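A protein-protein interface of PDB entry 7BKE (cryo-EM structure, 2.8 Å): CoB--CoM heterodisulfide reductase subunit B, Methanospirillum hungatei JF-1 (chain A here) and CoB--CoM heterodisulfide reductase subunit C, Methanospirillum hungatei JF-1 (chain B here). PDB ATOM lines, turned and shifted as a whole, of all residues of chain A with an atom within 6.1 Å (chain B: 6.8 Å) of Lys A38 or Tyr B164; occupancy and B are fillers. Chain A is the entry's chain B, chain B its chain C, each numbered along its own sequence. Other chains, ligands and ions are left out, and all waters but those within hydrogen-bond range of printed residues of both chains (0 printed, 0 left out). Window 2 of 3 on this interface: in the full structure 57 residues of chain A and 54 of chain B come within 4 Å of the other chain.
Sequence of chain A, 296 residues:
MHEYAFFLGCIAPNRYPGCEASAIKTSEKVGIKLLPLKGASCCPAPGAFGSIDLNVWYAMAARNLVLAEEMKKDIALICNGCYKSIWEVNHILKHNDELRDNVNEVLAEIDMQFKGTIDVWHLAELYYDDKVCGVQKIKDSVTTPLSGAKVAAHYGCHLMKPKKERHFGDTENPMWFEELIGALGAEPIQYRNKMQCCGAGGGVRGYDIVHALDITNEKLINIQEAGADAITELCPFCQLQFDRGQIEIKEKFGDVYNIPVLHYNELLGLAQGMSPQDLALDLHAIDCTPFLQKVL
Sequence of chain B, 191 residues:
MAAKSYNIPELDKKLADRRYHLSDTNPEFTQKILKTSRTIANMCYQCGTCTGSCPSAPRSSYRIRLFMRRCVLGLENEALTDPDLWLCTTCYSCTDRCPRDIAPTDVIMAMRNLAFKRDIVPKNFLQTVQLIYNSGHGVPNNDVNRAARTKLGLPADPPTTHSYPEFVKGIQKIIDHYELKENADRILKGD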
ATOM      1  N   PRO A  36       9.638  13.415  16.801  1.00  0.00           N
ATOM      2  CA  PRO A  36      10.747  12.687  17.429  1.00  0.00           C
ATOM      3  C   PRO A  36      11.339  13.459  18.598  1.00  0.00           C
ATOM      4  O   PRO A  36      11.453  14.684  18.567  1.00  0.00           O
ATOM      5  CB  PRO A  36      11.763  12.539  16.293  1.00  0.00           C
ATOM      6  CG  PRO A  36      10.974  12.697  15.045  1.00  0.00           C
ATOM      7  CD  PRO A  36       9.867  13.647  15.365  1.00  0.00           C
ATOM      8  N   LEU A  37      11.724  12.723  19.636  1.00  0.00           N
ATOM      9  CA  LEU A  37      12.424  13.303  20.771  1.00  0.00           C
ATOM     10  C   LEU A  37      13.919  13.240  20.506  1.00  0.00           C
ATOM     11  O   LEU A  37      14.441  12.194  20.113  1.00  0.00           O
ATOM     12  CB  LEU A  37      12.078  12.573  22.067  1.00  0.00           C
ATOM     13  CG  LEU A  37      12.258  13.391  23.343  1.00  0.00           C
ATOM     14  CD1 LEU A  37      11.737  14.789  23.149  1.00  0.00           C
ATOM     15  CD2 LEU A  37      11.549  12.726  24.494  1.00  0.00           C
ATOM     16  N   LYS A  38      14.602  14.358  20.722  1.00  0.00           N
ATOM     17  CA  LYS A  38      15.972  14.530  20.249  1.00  0.00           C
ATOM     18  C   LYS A  38      16.938  13.984  21.287  1.00  0.00           C
ATOM     19  O   LYS A  38      17.217  14.630  22.296  1.00  0.00           O
ATOM     20  CB  LYS A  38      16.241  16.002  19.960  1.00  0.00           C
ATOM     21  CG  LYS A  38      17.456  16.258  19.085  1.00  0.00           C
ATOM     22  CD  LYS A  38      17.382  15.446  17.796  1.00  0.00           C
ATOM     23  CE  LYS A  38      16.157  15.803  16.962  1.00  0.00           C
ATOM     24  NZ  LYS A  38      16.282  17.148  16.338  1.00  0.00           N
ATOM     25  N   GLY A  39      17.473  12.794  21.033  1.00  0.00           N
ATOM     26  CA  GLY A  39      18.439  12.217  21.942  1.00  0.00           C
ATOM     27  C   GLY A  39      17.867  11.664  23.225  1.00  0.00           C
ATOM     28  O   GLY A  39      18.587  11.582  24.223  1.00  0.00           O
ATOM     29  N   ALA A  40      16.593  11.290  23.235  1.00  0.00           N
ATOM     30  CA  ALA A  40      16.027  10.613  24.388  1.00  0.00           C
ATOM     31  C   ALA A  40      16.691   9.260  24.573  1.00  0.00           C
ATOM     32  O   ALA A  40      17.229   8.675  23.638  1.00  0.00           O
ATOM     33  CB  ALA A  40      14.522  10.433  24.225  1.00  0.00           C
ATOM     34  N   LEU A  67      14.557  17.348  27.983  1.00  0.00           N
ATOM     35  CA  LEU A  67      14.681  17.364  26.526  1.00  0.00           C
ATOM     36  C   LEU A  67      13.405  17.894  25.874  1.00  0.00           C
ATOM     37  O   LEU A  67      13.437  18.847  25.082  1.00  0.00           O
ATOM     38  CB  LEU A  67      14.991  15.964  26.010  1.00  0.00           C
ATOM     39  CG  LEU A  67      16.406  15.432  26.189  1.00  0.00           C
ATOM     40  CD1 LEU A  67      16.551  14.154  25.404  1.00  0.00           C
ATOM     41  CD2 LEU A  67      17.417  16.453  25.733  1.00  0.00           C
ATOM     42  N   MET A  71      12.263  21.343  23.926  1.00  0.00           N
ATOM     43  CA  MET A  71      11.435  21.286  22.726  1.00  0.00           C
ATOM     44  C   MET A  71      10.129  22.055  22.885  1.00  0.00           C
ATOM     45  O   MET A  71       9.488  22.379  21.880  1.00  0.00           O
ATOM     46  CB  MET A  71      11.138  19.834  22.359  1.00  0.00           C
ATOM     47  CG  MET A  71      10.727  19.627  20.922  1.00  0.00           C
ATOM     48  SD  MET A  71      10.514  17.886  20.523  1.00  0.00           S
ATOM     49  CE  MET A  71      12.113  17.517  19.818  1.00  0.00           C
ATOM     50  N   PRO B 158      16.940   4.514  15.756  1.00  0.00           N
ATOM     51  CA  PRO B 158      15.919   5.427  16.256  1.00  0.00           C
ATOM     52  C   PRO B 158      16.518   6.771  16.620  1.00  0.00           C
ATOM     53  O   PRO B 158      17.736   6.887  16.813  1.00  0.00           O
ATOM     54  CB  PRO B 158      15.377   4.699  17.496  1.00  0.00           C
ATOM     55  CG  PRO B 158      16.450   3.767  17.891  1.00  0.00           C
ATOM     56  CD  PRO B 158      17.111   3.343  16.627  1.00  0.00           C
ATOM     57  N   PRO B 159      15.689   7.813  16.735  1.00  0.00           N
ATOM     58  CA  PRO B 159      16.199   9.159  17.047  1.00  0.00           C
ATOM     59  C   PRO B 159      16.849   9.296  18.414  1.00  0.00           C
ATOM     60  O   PRO B 159      17.151  10.409  18.849  1.00  0.00           O
ATOM     61  CB  PRO B 159      14.942  10.038  16.952  1.00  0.00           C
ATOM     62  CG  PRO B 159      13.796   9.101  17.005  1.00  0.00           C
ATOM     63  CD  PRO B 159      14.262   7.838  16.385  1.00  0.00           C
ATOM     64  N   THR B 160      17.041   8.186  19.114  1.00  0.00           N
ATOM     65  CA  THR B 160      17.563   8.204  20.473  1.00  0.00           C
ATOM     66  C   THR B 160      19.075   8.400  20.528  1.00  0.00           C
ATOM     67  O   THR B 160      19.705   8.803  19.543  1.00  0.00           O
ATOM     68  CB  THR B 160      17.195   6.906  21.182  1.00  0.00           C
ATOM     69  OG1 THR B 160      17.876   5.816  20.558  1.00  0.00           O
ATOM     70  CG2 THR B 160      15.704   6.666  21.102  1.00  0.00           C
ATOM     71  N   THR B 161      19.664   8.132  21.695  1.00  0.00           N
ATOM     72  CA  THR B 161      21.114   8.179  21.831  1.00  0.00           C
ATOM     73  C   THR B 161      21.814   7.115  20.997  1.00  0.00           C
ATOM     74  O   THR B 161      23.046   7.086  20.977  1.00  0.00           O
ATOM     75  CB  THR B 161      21.524   8.024  23.295  1.00  0.00           C
ATOM     76  OG1 THR B 161      21.210   6.704  23.747  1.00  0.00           O
ATOM     77  CG2 THR B 161      20.808   9.032  24.161  1.00  0.00           C
ATOM     78  N   HIS B 162      21.064   6.233  20.333  1.00  0.00           N
ATOM     79  CA  HIS B 162      21.667   5.352  19.341  1.00  0.00           C
ATOM     80  C   HIS B 162      22.068   6.116  18.093  1.00  0.00           C
ATOM     81  O   HIS B 162      22.968   5.686  17.366  1.00  0.00           O
ATOM     82  CB  HIS B 162      20.703   4.232  18.963  1.00  0.00           C
ATOM     83  CG  HIS B 162      20.817   3.020  19.828  1.00  0.00           C
ATOM     84  ND1 HIS B 162      19.862   2.678  20.760  1.00  0.00           N
ATOM     85  CD2 HIS B 162      21.775   2.069  19.904  1.00  0.00           C
ATOM     86  CE1 HIS B 162      20.227   1.567  21.372  1.00  0.00           C
ATOM     87  NE2 HIS B 162      21.384   1.177  20.872  1.00  0.00           N
ATOM     88  N   SER B 163      21.400   7.229  17.814  1.00  0.00           N
ATOM     89  CA  SER B 163      21.737   8.063  16.676  1.00  0.00           C
ATOM     90  C   SER B 163      22.312   9.411  17.077  1.00  0.00           C
ATOM     91  O   SER B 163      22.796  10.138  16.208  1.00  0.00           O
ATOM     92  CB  SER B 163      20.504   8.281  15.793  1.00  0.00           C
ATOM     93  OG  SER B 163      19.644   9.247  16.363  1.00  0.00           O
ATOM     94  N   TYR B 164      22.269   9.765  18.361  1.00  0.00           N
ATOM     95  CA  TYR B 164      22.871  10.999  18.863  1.00  0.00           C
ATOM     96  C   TYR B 164      23.806  10.673  20.023  1.00  0.00           C
ATOM     97  O   TYR B 164      23.484  10.935  21.187  1.00  0.00           O
ATOM     98  CB  TYR B 164      21.800  11.998  19.284  1.00  0.00           C
ATOM     99  CG  TYR B 164      20.979  12.496  18.127  1.00  0.00           C
ATOM    100  CD1 TYR B 164      19.679  12.057  17.936  1.00  0.00           C
ATOM    101  CD2 TYR B 164      21.507  13.397  17.220  1.00  0.00           C
ATOM    102  CE1 TYR B 164      18.928  12.504  16.878  1.00  0.00           C
ATOM    103  CE2 TYR B 164      20.761  13.852  16.158  1.00  0.00           C
ATOM    104  CZ  TYR B 164      19.471  13.404  15.992  1.00  0.00           C
ATOM    105  OH  TYR B 164      18.722  13.855  14.935  1.00  0.00           O
ATOM    106  N   PRO B 165      24.989  10.125  19.731  1.00  0.00           N
ATOM    107  CA  PRO B 165      25.859   9.610  20.797  1.00  0.00           C
ATOM    108  C   PRO B 165      26.470  10.674  21.696  1.00  0.00           C
ATOM    109  O   PRO B 165      27.237  10.319  22.598  1.00  0.00           O
ATOM    110  CB  PRO B 165      26.956   8.862  20.020  1.00  0.00           C
ATOM    111  CG  PRO B 165      26.415   8.686  18.640  1.00  0.00           C
ATOM    112  CD  PRO B 165      25.546   9.866  18.399  1.00  0.00           C
ATOM    113  N   GLU B 166      26.188  11.958  21.490  1.00  0.00           N
ATOM    114  CA  GLU B 166      26.763  12.973  22.368  1.00  0.00           C
ATOM    115  C   GLU B 166      26.033  13.079  23.702  1.00  0.00           C
ATOM    116  O   GLU B 166      26.625  13.535  24.686  1.00  0.00           O
ATOM    117  CB  GLU B 166      26.801  14.327  21.658  1.00  0.00           C
ATOM    118  CG  GLU B 166      25.454  14.959  21.406  1.00  0.00           C
ATOM    119  CD  GLU B 166      24.813  14.460  20.129  1.00  0.00           C
ATOM    120  OE1 GLU B 166      25.262  13.423  19.597  1.00  0.00           O
ATOM    121  OE2 GLU B 166      23.854  15.104  19.654  1.00  0.00           O
ATOM    122  N   PHE B 167      24.764  12.672  23.769  1.00  0.00           N
ATOM    123  CA  PHE B 167      24.046  12.645  25.039  1.00  0.00           C
ATOM    124  C   PHE B 167      24.458  11.474  25.925  1.00  0.00           C
ATOM    125  O   PHE B 167      24.189  11.497  27.138  1.00  0.00           O
ATOM    126  CB  PHE B 167      22.541  12.587  24.795  1.00  0.00           C
ATOM    127  CG  PHE B 167      22.015  13.695  23.935  1.00  0.00           C
ATOM    128  CD1 PHE B 167      21.626  14.894  24.495  1.00  0.00           C
ATOM    129  CD2 PHE B 167      21.888  13.529  22.573  1.00  0.00           C
ATOM    130  CE1 PHE B 167      21.133  15.913  23.710  1.00  0.00           C
ATOM    131  CE2 PHE B 167      21.397  14.543  21.785  1.00  0.00           C
ATOM    132  CZ  PHE B 167      21.021  15.735  22.352  1.00  0.00           C
ATOM    133  N   VAL B 168      25.099  10.457  25.348  1.00  0.00           N
ATOM    134  CA  VAL B 168      25.556   9.320  26.136  1.00  0.00           C
ATOM    135  C   VAL B 168      26.533   9.785  27.198  1.00  0.00           C
ATOM    136  O   VAL B 168      26.545   9.271  28.319  1.00  0.00           O
ATOM    137  CB  VAL B 168      26.183   8.253  25.223  1.00  0.00           C
ATOM    138  CG1 VAL B 168      26.552   7.031  26.026  1.00  0.00           C
ATOM    139  CG2 VAL B 168      25.228   7.883  24.121  1.00  0.00           C
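The backbone carbonyl oxygen of Pro B159 sits close to the backbone carbonyl oxygen of Leu A37 (3.5 Å).
The backbone carbonyl oxygen (O) of Pro B159 sits at hydrogen-bond distance from the backbone NH (N) of Gly A39 (3.2 Å).
The backbone NH (N) of Thr B161 sits at hydrogen-bond distance from the backbone carbonyl oxygen (O) of Ala A40, at 3.2 Å.
The backbone carbonyl oxygen of Thr B160 sits at hydrogen-bond distance from the side-chain hydroxyl of Ser B163 (3.2 Å).
The side-chain hydroxyl (OG1) of Thr B160 sits close to the backbone NH (N) of His B162, 3.2 Å away.
Among the printed residues, merely in contact across the chains: Lys A38 with Tyr B164 (3.4 Å), Lys A38 with Phe B167 (3.96 Å), Gly A39 with Thr B161 (3.4 Å), Gly A39 with Tyr B164 (3.9 Å), Gly A39 with Phe B167 (3.7 Å) and Ala A40 with Thr B160 (3.0 Å).
Of the printed residues of chain B, Leu A37 touches Pro B159.
Lys A38 touches two residues of chain B.
Printed residues of chain A within 4 Å of Thr B161: Gly A39 and Ala A40.
Ser B163 touches none of the printed residues of chain A.
Tyr B164 touches just these residues of chain A: Lys A38 and Gly A39.
Of the printed residues of chain A, Phe B167 touches Lys A38 (3.96 Å) and Gly A39 (3.7 Å).
Val B168 touches none of the printed residues of chain A.
The nearest residue of chain A that does not touch Tyr B164 is Leu A37 (5.5 Å).
The nearest printed residue of chain A that does not touch Thr B160 is Gly A39 (4.1 Å).
Of the 11 printed residues of chain B, 5 touch a printed residue of chain A.
Hydrophobic or aromatic side chains of chain B within 4 Å of the printed part of chain A: Pro B159, Tyr B164 and Phe B167.
Of the 7 printed residues of chain A, 4 touch a printed residue of chain B.
Among the printed residues, 9 pairs touch across the chains.
Among the printed residues, no Asp or Glu carboxylate lies within 4 Å of a Lys or Arg side-chain nitrogen of the other chain.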
